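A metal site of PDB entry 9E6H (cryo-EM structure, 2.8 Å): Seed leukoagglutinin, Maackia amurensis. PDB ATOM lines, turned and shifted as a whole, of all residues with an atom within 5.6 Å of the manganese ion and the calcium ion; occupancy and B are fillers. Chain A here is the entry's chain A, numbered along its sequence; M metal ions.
Four residues have an atom within 4 Å of the manganese ion: Glu 156, Asp 158, Asp 169 and His 174. The nearest printed residue that does not touch the manganese ion is Ser 184 (4.5 Å).
The backbone NH (N) of Asp 158 lies within hydrogen-bond range of the backbone carbonyl oxygen (O) of His 174 (2.9 Å). The side-chain carboxylate (OE2) of Glu 156 lies close to the side-chain hydroxyl (OG) of Ser 184 (3.0 Å).
The calcium ion is bound by O of Tyr 160 (2.3 Å), OD2 of Asp 169 (2.4 Å), OD1 of Asp 158 (2.4 Å), OD2 of Asp 158 (2.4 Å) and OD2 of Asp 166 (2.4 Å).
The manganese ion is bound by the side-chain carboxylate (OD1) of Asp 169 (2.1 Å), the side-chain carboxylate (OE2) of Glu 156 (2.1 Å) and a ring nitrogen (NE2) of His 174 (2.2 Å). The manganese ion has three donor atoms within binding distance.
Of the 16 residues printed, 4 come within 4 Å of the calcium ion.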
ATOM      1  N   ASP A 116      -3.268  -4.600  -1.931  1.00  0.00           N
ATOM      2  CA  ASP A 116      -4.127  -5.762  -2.144  1.00  0.00           C
ATOM      3  C   ASP A 116      -3.680  -6.951  -1.300  1.00  0.00           C
ATOM      4  O   ASP A 116      -3.801  -6.908  -0.068  1.00  0.00           O
ATOM      5  CB  ASP A 116      -4.154  -6.112  -3.631  1.00  0.00           C
ATOM      6  CG  ASP A 116      -4.818  -5.042  -4.467  1.00  0.00           C
ATOM      7  OD1 ASP A 116      -5.702  -4.325  -3.945  1.00  0.00           O
ATOM      8  OD2 ASP A 116      -4.451  -4.896  -5.654  1.00  0.00           O
ATOM      9  N   LYS A 136      -8.321  -4.600  -6.459  1.00  0.00           N
ATOM     10  CA  LYS A 136      -8.856  -4.544  -5.106  1.00  0.00           C
ATOM     11  C   LYS A 136      -9.653  -5.784  -4.729  1.00  0.00           C
ATOM     12  O   LYS A 136      -9.920  -5.979  -3.531  1.00  0.00           O
ATOM     13  CB  LYS A 136      -9.732  -3.288  -4.948  1.00  0.00           C
ATOM     14  CG  LYS A 136     -10.993  -3.282  -5.807  1.00  0.00           C
ATOM     15  CD  LYS A 136     -11.839  -2.044  -5.584  1.00  0.00           C
ATOM     16  CE  LYS A 136     -11.205  -0.794  -6.173  1.00  0.00           C
ATOM     17  NZ  LYS A 136     -11.142  -0.834  -7.655  1.00  0.00           N
ATOM     18  N   GLU A 156      -8.628 -15.136   2.285  1.00  0.00           N
ATOM     19  CA  GLU A 156      -7.805 -14.031   1.844  1.00  0.00           C
ATOM     20  C   GLU A 156      -6.934 -13.515   2.980  1.00  0.00           C
ATOM     21  O   GLU A 156      -7.347 -13.475   4.137  1.00  0.00           O
ATOM     22  CB  GLU A 156      -8.665 -12.891   1.294  1.00  0.00           C
ATOM     23  CG  GLU A 156      -9.462 -12.120   2.342  1.00  0.00           C
ATOM     24  CD  GLU A 156     -10.266 -10.980   1.734  1.00  0.00           C
ATOM     25  OE1 GLU A 156     -10.360 -10.913   0.491  1.00  0.00           O
ATOM     26  OE2 GLU A 156     -10.796 -10.149   2.503  1.00  0.00           O
ATOM     27  N   ASP A 158      -5.636 -10.158   3.450  1.00  0.00           N
ATOM     28  CA  ASP A 158      -5.752  -8.806   2.930  1.00  0.00           C
ATOM     29  C   ASP A 158      -4.844  -7.882   3.731  1.00  0.00           C
ATOM     30  O   ASP A 158      -5.006  -7.732   4.948  1.00  0.00           O
ATOM     31  CB  ASP A 158      -7.198  -8.316   2.996  1.00  0.00           C
ATOM     32  CG  ASP A 158      -7.417  -7.018   2.239  1.00  0.00           C
ATOM     33  OD1 ASP A 158      -6.943  -5.966   2.720  1.00  0.00           O
ATOM     34  OD2 ASP A 158      -8.067  -7.041   1.174  1.00  0.00           O
ATOM     35  N   THR A 159      -3.890  -7.263   3.030  1.00  0.00           N
ATOM     36  CA  THR A 159      -2.924  -6.353   3.640  1.00  0.00           C
ATOM     37  C   THR A 159      -3.255  -4.891   3.384  1.00  0.00           C
ATOM     38  O   THR A 159      -2.551  -4.016   3.906  1.00  0.00           O
ATOM     39  CB  THR A 159      -1.517  -6.650   3.108  1.00  0.00           C
ATOM     40  OG1 THR A 159      -1.476  -6.430   1.697  1.00  0.00           O
ATOM     41  CG2 THR A 159      -1.139  -8.099   3.394  1.00  0.00           C
ATOM     42  N   TYR A 160      -4.294  -4.595   2.605  1.00  0.00           N
ATOM     43  CA  TYR A 160      -4.691  -3.236   2.275  1.00  0.00           C
ATOM     44  C   TYR A 160      -5.975  -2.914   3.034  1.00  0.00           C
ATOM     45  O   TYR A 160      -7.020  -3.538   2.799  1.00  0.00           O
ATOM     46  CB  TYR A 160      -4.887  -3.072   0.772  1.00  0.00           C
ATOM     47  CG  TYR A 160      -5.165  -1.645   0.325  1.00  0.00           C
ATOM     48  CD1 TYR A 160      -4.332  -0.604   0.710  1.00  0.00           C
ATOM     49  CD2 TYR A 160      -6.261  -1.359  -0.481  1.00  0.00           C
ATOM     50  CE1 TYR A 160      -4.588   0.690   0.305  1.00  0.00           C
ATOM     51  CE2 TYR A 160      -6.517  -0.065  -0.887  1.00  0.00           C
ATOM     52  CZ  TYR A 160      -5.677   0.960  -0.500  1.00  0.00           C
ATOM     53  OH  TYR A 160      -5.935   2.241  -0.901  1.00  0.00           O
ATOM     54  N   PHE A 161      -5.903  -1.941   3.952  1.00  0.00           N
ATOM     55  CA  PHE A 161      -7.021  -1.577   4.800  1.00  0.00           C
ATOM     56  C   PHE A 161      -7.663  -0.259   4.377  1.00  0.00           C
ATOM     57  O   PHE A 161      -8.310   0.402   5.197  1.00  0.00           O
ATOM     58  CB  PHE A 161      -6.580  -1.497   6.274  1.00  0.00           C
ATOM     59  CG  PHE A 161      -5.201  -0.934   6.474  1.00  0.00           C
ATOM     60  CD1 PHE A 161      -5.005   0.435   6.583  1.00  0.00           C
ATOM     61  CD2 PHE A 161      -4.102  -1.773   6.542  1.00  0.00           C
ATOM     62  CE1 PHE A 161      -3.734   0.947   6.768  1.00  0.00           C
ATOM     63  CE2 PHE A 161      -2.828  -1.253   6.731  1.00  0.00           C
ATOM     64  CZ  PHE A 161      -2.645   0.109   6.840  1.00  0.00           C
ATOM     65  N   GLY A 162      -7.491   0.141   3.123  1.00  0.00           N
ATOM     66  CA  GLY A 162      -8.036   1.405   2.673  1.00  0.00           C
ATOM     67  C   GLY A 162      -9.550   1.450   2.809  1.00  0.00           C
ATOM     68  O   GLY A 162     -10.240   0.443   2.663  1.00  0.00           O
ATOM     69  N   ASP A 166     -11.586   0.264  -0.480  1.00  0.00           N
ATOM     70  CA  ASP A 166     -12.074  -0.967   0.132  1.00  0.00           C
ATOM     71  C   ASP A 166     -12.917  -0.608   1.343  1.00  0.00           C
ATOM     72  O   ASP A 166     -12.516  -0.877   2.494  1.00  0.00           O
ATOM     73  CB  ASP A 166     -10.924  -1.900   0.531  1.00  0.00           C
ATOM     74  CG  ASP A 166     -10.160  -2.441  -0.665  1.00  0.00           C
ATOM     75  OD1 ASP A 166     -10.434  -2.010  -1.805  1.00  0.00           O
ATOM     76  OD2 ASP A 166      -9.281  -3.302  -0.457  1.00  0.00           O
ATOM     77  N   TRP A 168     -15.543  -2.045   2.384  1.00  0.00           N
ATOM     78  CA  TRP A 168     -15.993  -3.259   3.055  1.00  0.00           C
ATOM     79  C   TRP A 168     -14.959  -3.791   4.034  1.00  0.00           C
ATOM     80  O   TRP A 168     -15.326  -4.315   5.092  1.00  0.00           O
ATOM     81  CB  TRP A 168     -16.346  -4.342   2.026  1.00  0.00           C
ATOM     82  CG  TRP A 168     -15.235  -4.652   1.058  1.00  0.00           C
ATOM     83  CD1 TRP A 168     -14.225  -5.541   1.223  1.00  0.00           C
ATOM     84  CD2 TRP A 168     -15.040  -4.047  -0.231  1.00  0.00           C
ATOM     85  NE1 TRP A 168     -13.407  -5.548   0.122  1.00  0.00           N
ATOM     86  CE2 TRP A 168     -13.884  -4.642  -0.795  1.00  0.00           C
ATOM     87  CE3 TRP A 168     -15.720  -3.081  -0.969  1.00  0.00           C
ATOM     88  CZ2 TRP A 168     -13.403  -4.285  -2.046  1.00  0.00           C
ATOM     89  CZ3 TRP A 168     -15.242  -2.737  -2.215  1.00  0.00           C
ATOM     90  CH2 TRP A 168     -14.094  -3.333  -2.742  1.00  0.00           C
ATOM     91  N   ASP A 169     -13.673  -3.687   3.703  1.00  0.00           N
ATOM     92  CA  ASP A 169     -12.635  -4.237   4.557  1.00  0.00           C
ATOM     93  C   ASP A 169     -12.540  -3.453   5.865  1.00  0.00           C
ATOM     94  O   ASP A 169     -12.850  -2.251   5.894  1.00  0.00           O
ATOM     95  CB  ASP A 169     -11.292  -4.220   3.847  1.00  0.00           C
ATOM     96  CG  ASP A 169     -11.083  -5.426   2.942  1.00  0.00           C
ATOM     97  OD1 ASP A 169     -11.686  -6.493   3.205  1.00  0.00           O
ATOM     98  OD2 ASP A 169     -10.318  -5.309   1.962  1.00  0.00           O
ATOM     99  N   PRO A 170     -12.120  -4.096   6.966  1.00  0.00           N
ATOM    100  CA  PRO A 170     -11.934  -3.352   8.222  1.00  0.00           C
ATOM    101  C   PRO A 170     -10.751  -2.388   8.179  1.00  0.00           C
ATOM    102  O   PRO A 170     -10.078  -2.256   7.148  1.00  0.00           O
ATOM    103  CB  PRO A 170     -11.708  -4.464   9.246  1.00  0.00           C
ATOM    104  CG  PRO A 170     -11.207  -5.617   8.466  1.00  0.00           C
ATOM    105  CD  PRO A 170     -11.920  -5.542   7.155  1.00  0.00           C
ATOM    106  N   HIS A 174      -5.923  -7.869   7.755  1.00  0.00           N
ATOM    107  CA  HIS A 174      -6.793  -8.926   8.243  1.00  0.00           C
ATOM    108  C   HIS A 174      -6.650 -10.198   7.421  1.00  0.00           C
ATOM    109  O   HIS A 174      -6.119 -10.192   6.308  1.00  0.00           O
ATOM    110  CB  HIS A 174      -8.262  -8.468   8.240  1.00  0.00           C
ATOM    111  CG  HIS A 174      -8.714  -7.881   6.945  1.00  0.00           C
ATOM    112  ND1 HIS A 174      -8.353  -6.622   6.535  1.00  0.00           N
ATOM    113  CD2 HIS A 174      -9.526  -8.364   5.973  1.00  0.00           C
ATOM    114  CE1 HIS A 174      -8.899  -6.360   5.355  1.00  0.00           C
ATOM    115  NE2 HIS A 174      -9.621  -7.404   5.002  1.00  0.00           N
ATOM    116  N   ILE A 182     -16.478 -10.414  -2.186  1.00  0.00           N
ATOM    117  CA  ILE A 182     -15.286  -9.857  -1.558  1.00  0.00           C
ATOM    118  C   ILE A 182     -15.521  -9.564  -0.078  1.00  0.00           C
ATOM    119  O   ILE A 182     -14.594  -9.705   0.726  1.00  0.00           O
ATOM    120  CB  ILE A 182     -14.836  -8.587  -2.303  1.00  0.00           C
ATOM    121  CG1 ILE A 182     -13.432  -8.159  -1.869  1.00  0.00           C
ATOM    122  CG2 ILE A 182     -15.822  -7.452  -2.081  1.00  0.00           C
ATOM    123  CD1 ILE A 182     -12.341  -9.142  -2.253  1.00  0.00           C
ATOM    124  N   SER A 184     -15.899 -10.270   3.313  1.00  0.00           N
ATOM    125  CA  SER A 184     -15.670 -11.492   4.073  1.00  0.00           C
ATOM    126  C   SER A 184     -16.694 -11.644   5.183  1.00  0.00           C
ATOM    127  O   SER A 184     -16.998 -10.694   5.906  1.00  0.00           O
ATOM    128  CB  SER A 184     -14.256 -11.476   4.669  1.00  0.00           C
ATOM    129  OG  SER A 184     -13.277 -11.482   3.647  1.00  0.00           O
ATOM    130  N   THR A 187     -13.582 -12.098   9.667  1.00  0.00           N
ATOM    131  CA  THR A 187     -12.200 -11.625   9.554  1.00  0.00           C
ATOM    132  C   THR A 187     -11.558 -11.603  10.931  1.00  0.00           C
ATOM    133  O   THR A 187     -12.228 -11.473  11.949  1.00  0.00           O
ATOM    134  CB  THR A 187     -12.143 -10.223   8.930  1.00  0.00           C
ATOM    135  OG1 THR A 187     -12.885  -9.306   9.743  1.00  0.00           O
ATOM    136  CG2 THR A 187     -12.712 -10.233   7.532  1.00  0.00           C
HETATM  137 MN    MN M   1     -10.306  -8.126   3.028  1.00  0.00          MN
HETATM  138 CA    CA M   2      -8.187  -4.667   1.177  1.00  0.00          CA
